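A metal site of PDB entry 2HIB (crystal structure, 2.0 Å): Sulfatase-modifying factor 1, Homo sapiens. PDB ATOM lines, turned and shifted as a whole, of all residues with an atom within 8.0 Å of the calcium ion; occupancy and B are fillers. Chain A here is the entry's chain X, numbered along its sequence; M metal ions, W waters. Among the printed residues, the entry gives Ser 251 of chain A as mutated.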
ATOM      1  N   HIS A 171       5.654  30.033  17.855  1.00  0.00           N
ATOM      2  CA  HIS A 171       5.985  30.200  19.269  1.00  0.00           C
ATOM      3  C   HIS A 171       7.237  29.402  19.615  1.00  0.00           C
ATOM      4  O   HIS A 171       7.350  28.220  19.272  1.00  0.00           O
ATOM      5  CB  HIS A 171       4.821  29.812  20.163  1.00  0.00           C
ATOM      6  CG  HIS A 171       3.724  30.817  20.183  1.00  0.00           C
ATOM      7  ND1 HIS A 171       3.800  31.987  20.905  1.00  0.00           N
ATOM      8  CD2 HIS A 171       2.540  30.855  19.524  1.00  0.00           C
ATOM      9  CE1 HIS A 171       2.710  32.685  20.708  1.00  0.00           C
ATOM     10  NE2 HIS A 171       1.920  32.020  19.885  1.00  0.00           N
ATOM     11  N   ALA A 173       8.603  29.618  22.940  1.00  0.00           N
ATOM     12  CA  ALA A 173       8.664  29.455  24.393  1.00  0.00           C
ATOM     13  C   ALA A 173       7.284  29.525  25.035  1.00  0.00           C
ATOM     14  O   ALA A 173       6.347  30.097  24.488  1.00  0.00           O
ATOM     15  CB  ALA A 173       9.617  30.504  25.032  1.00  0.00           C
ATOM     16  N   ASN A 174       7.203  28.937  26.224  1.00  0.00           N
ATOM     17  CA  ASN A 174       5.972  28.956  27.008  1.00  0.00           C
ATOM     18  C   ASN A 174       5.950  30.186  27.946  1.00  0.00           C
ATOM     19  O   ASN A 174       6.517  30.171  29.034  1.00  0.00           O
ATOM     20  CB  ASN A 174       5.802  27.657  27.778  1.00  0.00           C
ATOM     21  CG  ASN A 174       4.468  27.602  28.520  1.00  0.00           C
ATOM     22  OD1 ASN A 174       3.568  28.393  28.226  1.00  0.00           O
ATOM     23  ND2 ASN A 174       4.355  26.721  29.501  1.00  0.00           N
ATOM     24  N   ILE A 175       5.306  31.259  27.467  1.00  0.00           N
ATOM     25  CA  ILE A 175       5.036  32.448  28.292  1.00  0.00           C
ATOM     26  C   ILE A 175       3.529  32.761  28.256  1.00  0.00           C
ATOM     27  O   ILE A 175       2.696  31.885  27.945  1.00  0.00           O
ATOM     28  CB  ILE A 175       5.973  33.609  27.881  1.00  0.00           C
ATOM     29  CG1 ILE A 175       5.674  34.118  26.459  1.00  0.00           C
ATOM     30  CG2 ILE A 175       7.431  33.133  27.964  1.00  0.00           C
ATOM     31  CD1 ILE A 175       6.430  35.387  26.074  1.00  0.00           C
ATOM     32  N   TRP A 176       3.143  33.987  28.581  1.00  0.00           N
ATOM     33  CA  TRP A 176       1.750  34.370  28.700  1.00  0.00           C
ATOM     34  C   TRP A 176       1.324  35.065  27.413  1.00  0.00           C
ATOM     35  O   TRP A 176       2.067  35.873  26.850  1.00  0.00           O
ATOM     36  CB  TRP A 176       1.578  35.322  29.877  1.00  0.00           C
ATOM     37  CG  TRP A 176       0.183  35.761  30.210  1.00  0.00           C
ATOM     38  CD1 TRP A 176      -0.584  36.662  29.532  1.00  0.00           C
ATOM     39  CD2 TRP A 176      -0.597  35.335  31.328  1.00  0.00           C
ATOM     40  NE1 TRP A 176      -1.806  36.829  30.162  1.00  0.00           N
ATOM     41  CE2 TRP A 176      -1.830  36.017  31.259  1.00  0.00           C
ATOM     42  CE3 TRP A 176      -0.365  34.435  32.369  1.00  0.00           C
ATOM     43  CZ2 TRP A 176      -2.835  35.835  32.225  1.00  0.00           C
ATOM     44  CZ3 TRP A 176      -1.365  34.247  33.320  1.00  0.00           C
ATOM     45  CH2 TRP A 176      -2.580  34.951  33.242  1.00  0.00           C
ATOM     46  N   GLN A 177       0.132  34.731  26.919  1.00  0.00           N
ATOM     47  CA  GLN A 177      -0.518  35.561  25.908  1.00  0.00           C
ATOM     48  C   GLN A 177      -1.843  36.056  26.450  1.00  0.00           C
ATOM     49  O   GLN A 177      -2.560  35.315  27.104  1.00  0.00           O
ATOM     50  CB  GLN A 177      -0.757  34.800  24.600  1.00  0.00           C
ATOM     51  CG  GLN A 177       0.503  34.376  23.859  1.00  0.00           C
ATOM     52  CD  GLN A 177       1.013  33.043  24.336  1.00  0.00           C
ATOM     53  OE1 GLN A 177       0.232  32.097  24.555  1.00  0.00           O
ATOM     54  NE2 GLN A 177       2.345  32.943  24.490  1.00  0.00           N
ATOM     55  N   ASN A 184      -5.193  34.434  30.230  1.00  0.00           N
ATOM     56  CA  ASN A 184      -4.151  33.720  29.492  1.00  0.00           C
ATOM     57  C   ASN A 184      -4.861  32.916  28.410  1.00  0.00           C
ATOM     58  O   ASN A 184      -5.637  31.996  28.699  1.00  0.00           O
ATOM     59  CB  ASN A 184      -3.354  32.800  30.418  1.00  0.00           C
ATOM     60  CG  ASN A 184      -2.090  32.269  29.776  1.00  0.00           C
ATOM     61  OD1 ASN A 184      -1.869  32.440  28.584  1.00  0.00           O
ATOM     62  ND2 ASN A 184      -1.247  31.597  30.556  1.00  0.00           N
ATOM     63  N   THR A 185      -4.606  33.281  27.157  1.00  0.00           N
ATOM     64  CA  THR A 185      -5.297  32.668  26.029  1.00  0.00           C
ATOM     65  C   THR A 185      -4.832  31.243  25.755  1.00  0.00           C
ATOM     66  O   THR A 185      -5.540  30.477  25.122  1.00  0.00           O
ATOM     67  CB  THR A 185      -5.178  33.501  24.732  1.00  0.00           C
ATOM     68  OG1 THR A 185      -3.808  33.596  24.334  1.00  0.00           O
ATOM     69  CG2 THR A 185      -5.765  34.908  24.914  1.00  0.00           C
ATOM     70  N   GLY A 186      -3.620  30.885  26.195  1.00  0.00           N
ATOM     71  CA  GLY A 186      -3.085  29.577  25.846  1.00  0.00           C
ATOM     72  C   GLY A 186      -2.719  29.429  24.379  1.00  0.00           C
ATOM     73  O   GLY A 186      -2.660  28.304  23.838  1.00  0.00           O
ATOM     74  N   GLU A 187      -2.474  30.569  23.727  1.00  0.00           N
ATOM     75  CA  GLU A 187      -2.145  30.589  22.295  1.00  0.00           C
ATOM     76  C   GLU A 187      -0.935  29.707  21.975  1.00  0.00           C
ATOM     77  O   GLU A 187      -0.896  29.027  20.940  1.00  0.00           O
ATOM     78  CB  GLU A 187      -1.873  32.038  21.837  1.00  0.00           C
ATOM     79  CG  GLU A 187      -1.583  32.207  20.350  1.00  0.00           C
ATOM     80  CD  GLU A 187      -1.034  33.596  20.005  1.00  0.00           C
ATOM     81  OE1 GLU A 187      -1.520  34.606  20.581  1.00  0.00           O
ATOM     82  OE2 GLU A 187      -0.130  33.664  19.174  1.00  0.00           O
ATOM     83  N   ASP A 188       0.033  29.673  22.881  1.00  0.00           N
ATOM     84  CA  ASP A 188       1.253  28.922  22.584  1.00  0.00           C
ATOM     85  C   ASP A 188       1.122  27.415  22.880  1.00  0.00           C
ATOM     86  O   ASP A 188       2.085  26.677  22.720  1.00  0.00           O
ATOM     87  CB  ASP A 188       2.457  29.540  23.288  1.00  0.00           C
ATOM     88  CG  ASP A 188       2.344  29.523  24.782  1.00  0.00           C
ATOM     89  OD1 ASP A 188       1.524  28.764  25.337  1.00  0.00           O
ATOM     90  OD2 ASP A 188       3.101  30.286  25.430  1.00  0.00           O
ATOM     91  N   GLY A 189      -0.072  26.992  23.337  1.00  0.00           N
ATOM     92  CA  GLY A 189      -0.402  25.584  23.556  1.00  0.00           C
ATOM     93  C   GLY A 189      -0.444  25.167  25.032  1.00  0.00           C
ATOM     94  O   GLY A 189      -0.812  24.028  25.333  1.00  0.00           O
ATOM     95  N   PHE A 190      -0.048  26.078  25.932  1.00  0.00           N
ATOM     96  CA  PHE A 190       0.014  25.825  27.365  1.00  0.00           C
ATOM     97  C   PHE A 190      -0.298  27.054  28.189  1.00  0.00           C
ATOM     98  O   PHE A 190       0.303  28.110  27.995  1.00  0.00           O
ATOM     99  CB  PHE A 190       1.415  25.302  27.750  1.00  0.00           C
ATOM    100  CG  PHE A 190       1.874  24.173  26.883  1.00  0.00           C
ATOM    101  CD1 PHE A 190       1.534  22.865  27.211  1.00  0.00           C
ATOM    102  CD2 PHE A 190       2.573  24.430  25.704  1.00  0.00           C
ATOM    103  CE1 PHE A 190       1.931  21.800  26.374  1.00  0.00           C
ATOM    104  CE2 PHE A 190       2.968  23.379  24.862  1.00  0.00           C
ATOM    105  CZ  PHE A 190       2.639  22.057  25.191  1.00  0.00           C
ATOM    106  N   GLN A 191      -1.229  26.906  29.121  1.00  0.00           N
ATOM    107  CA  GLN A 191      -1.546  27.972  30.081  1.00  0.00           C
ATOM    108  C   GLN A 191      -0.620  27.895  31.297  1.00  0.00           C
ATOM    109  O   GLN A 191       0.032  28.890  31.662  1.00  0.00           O
ATOM    110  CB  GLN A 191      -3.020  27.868  30.490  1.00  0.00           C
ATOM    111  CG  GLN A 191      -3.916  28.321  29.358  1.00  0.00           C
ATOM    112  CD  GLN A 191      -5.360  28.094  29.627  1.00  0.00           C
ATOM    113  OE1 GLN A 191      -5.768  26.990  30.018  1.00  0.00           O
ATOM    114  NE2 GLN A 191      -6.162  29.134  29.379  1.00  0.00           N
ATOM    115  N   GLY A 192      -0.545  26.712  31.890  1.00  0.00           N
ATOM    116  CA  GLY A 192       0.442  26.429  32.916  1.00  0.00           C
ATOM    117  C   GLY A 192       1.728  25.973  32.243  1.00  0.00           C
ATOM    118  O   GLY A 192       2.123  26.477  31.178  1.00  0.00           O
ATOM    119  N   THR A 193       2.388  24.991  32.841  1.00  0.00           N
ATOM    120  CA  THR A 193       3.637  24.465  32.301  1.00  0.00           C
ATOM    121  C   THR A 193       3.398  23.592  31.081  1.00  0.00           C
ATOM    122  O   THR A 193       2.281  23.096  30.821  1.00  0.00           O
ATOM    123  CB  THR A 193       4.414  23.647  33.364  1.00  0.00           C
ATOM    124  OG1 THR A 193       3.561  22.617  33.874  1.00  0.00           O
ATOM    125  CG2 THR A 193       4.853  24.545  34.545  1.00  0.00           C
ATOM    126  N   ALA A 194       4.493  23.415  30.342  1.00  0.00           N
ATOM    127  CA  ALA A 194       4.572  22.463  29.258  1.00  0.00           C
ATOM    128  C   ALA A 194       5.539  21.353  29.633  1.00  0.00           C
ATOM    129  O   ALA A 194       6.366  21.525  30.549  1.00  0.00           O
ATOM    130  CB  ALA A 194       5.043  23.144  27.966  1.00  0.00           C
ATOM    131  N   PHE A 199       8.807  22.740  22.692  1.00  0.00           N
ATOM    132  CA  PHE A 199       9.327  23.901  21.948  1.00  0.00           C
ATOM    133  C   PHE A 199      10.732  23.634  21.378  1.00  0.00           C
ATOM    134  O   PHE A 199      11.394  22.696  21.786  1.00  0.00           O
ATOM    135  CB  PHE A 199       9.268  25.189  22.787  1.00  0.00           C
ATOM    136  CG  PHE A 199       7.868  25.611  23.136  1.00  0.00           C
ATOM    137  CD1 PHE A 199       7.072  26.284  22.199  1.00  0.00           C
ATOM    138  CD2 PHE A 199       7.316  25.308  24.366  1.00  0.00           C
ATOM    139  CE1 PHE A 199       5.762  26.664  22.506  1.00  0.00           C
ATOM    140  CE2 PHE A 199       6.011  25.670  24.687  1.00  0.00           C
ATOM    141  CZ  PHE A 199       5.231  26.357  23.762  1.00  0.00           C
ATOM    142  N   ASN A 212       8.391  28.753  30.559  1.00  0.00           N
ATOM    143  CA  ASN A 212       8.006  27.549  31.268  1.00  0.00           C
ATOM    144  C   ASN A 212       8.173  27.703  32.784  1.00  0.00           C
ATOM    145  O   ASN A 212       7.299  28.304  33.405  1.00  0.00           O
ATOM    146  CB  ASN A 212       8.686  26.291  30.677  1.00  0.00           C
ATOM    147  CG  ASN A 212       7.778  25.067  30.720  1.00  0.00           C
ATOM    148  OD1 ASN A 212       6.557  25.197  30.713  1.00  0.00           O
ATOM    149  ND2 ASN A 212       8.375  23.857  30.721  1.00  0.00           N
ATOM    150  N   SER A 248       9.040  32.636  33.022  1.00  0.00           N
ATOM    151  CA  SER A 248       8.126  31.529  33.238  1.00  0.00           C
ATOM    152  C   SER A 248       6.928  31.653  32.345  1.00  0.00           C
ATOM    153  O   SER A 248       6.792  32.623  31.604  1.00  0.00           O
ATOM    154  CB  SER A 248       7.634  31.528  34.694  1.00  0.00           C
ATOM    155  OG  SER A 248       6.525  32.411  34.883  1.00  0.00           O
ATOM    156  N   TYR A 249       6.024  30.679  32.469  1.00  0.00           N
ATOM    157  CA  TYR A 249       4.804  30.662  31.692  1.00  0.00           C
ATOM    158  C   TYR A 249       3.894  31.871  32.018  1.00  0.00           C
ATOM    159  O   TYR A 249       2.900  32.135  31.313  1.00  0.00           O
ATOM    160  CB  TYR A 249       4.076  29.339  31.901  1.00  0.00           C
ATOM    161  CG  TYR A 249       3.537  29.107  33.301  1.00  0.00           C
ATOM    162  CD1 TYR A 249       2.351  29.701  33.697  1.00  0.00           C
ATOM    163  CD2 TYR A 249       4.171  28.253  34.189  1.00  0.00           C
ATOM    164  CE1 TYR A 249       1.814  29.480  34.961  1.00  0.00           C
ATOM    165  CE2 TYR A 249       3.629  28.014  35.470  1.00  0.00           C
ATOM    166  CZ  TYR A 249       2.460  28.633  35.826  1.00  0.00           C
ATOM    167  OH  TYR A 249       1.901  28.429  37.059  1.00  0.00           O
ATOM    168  N   MET A 250       4.225  32.567  33.098  1.00  0.00           N
ATOM    169  CA  MET A 250       3.511  33.792  33.487  1.00  0.00           C
ATOM    170  C   MET A 250       4.062  35.070  32.845  1.00  0.00           C
ATOM    171  O   MET A 250       3.393  36.088  32.863  1.00  0.00           O
ATOM    172  CB  MET A 250       3.509  33.951  35.010  1.00  0.00           C
ATOM    173  CG  MET A 250       2.647  32.940  35.720  1.00  0.00           C
ATOM    174  SD  MET A 250       2.961  32.978  37.487  1.00  0.00           S
ATOM    175  CE  MET A 250       2.094  34.534  37.880  1.00  0.00           C
ATOM    176  N   SER A 251       5.239  35.002  32.232  1.00  0.00           N
ATOM    177  CA  SER A 251       5.893  36.186  31.752  1.00  0.00           C
ATOM    178  C   SER A 251       5.177  36.810  30.551  1.00  0.00           C
ATOM    179  O   SER A 251       4.600  36.099  29.697  1.00  0.00           O
ATOM    180  CB  SER A 251       7.364  35.913  31.411  1.00  0.00           C
ATOM    181  OG  SER A 251       8.071  35.346  32.502  1.00  0.00           O
HETATM  182 CA    CA M   1       1.818  29.792  27.556  1.00  0.00          CA
HETATM  183  O   HOH W   1       1.303  30.299  29.901  1.00  0.00           O
HETATM  184  O   HOH W   2      -0.124  31.068  27.005  1.00  0.00           O
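ND2 of Asn 174 is in hydrogen-bond range of O of Gly 192 (2.8 Å).
The backbone carbonyl oxygen of Asn 174 sits at hydrogen-bond distance from the backbone NH of Asn 212 (2.8 Å).
The side-chain amide nitrogen (ND2) of Asn 174 sits close to the backbone NH (N) of Ala 194 (3.4 Å).
N of Asp 188 is in hydrogen-bond range of OE1 of Gln 177, 3.0 Å away.
Within 4 Å of the calcium ion: Asn 174, Ile 175, Asp 188 and Phe 190.
The calcium ion is bound by O of Ile 175 (2.3 Å).
The backbone carbonyl oxygen (O) of Phe 190 binds the calcium ion, 2.3 Å away.
The calcium ion is bound by the side-chain amide oxygen (OD1) of Asn 174 (2.3 Å).
The calcium ion is bound by water W2, 2.4 Å away.
Water W1 binds the calcium ion (2.5 Å).
The calcium ion is bound by OD1 of Asp 188 (2.5 Å).
OD2 of Asp 188 is bound to the calcium ion (2.5 Å).
Water W1 lies within hydrogen-bond range of O of Gln 191 (2.6 Å), O of Tyr 249 (2.8 Å) and ND2 of Asn 184 (2.9 Å).
Water W2 bridges OE1 of Gln 177 (2.7 Å) and OD1 of Asn 184 (2.7 Å).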
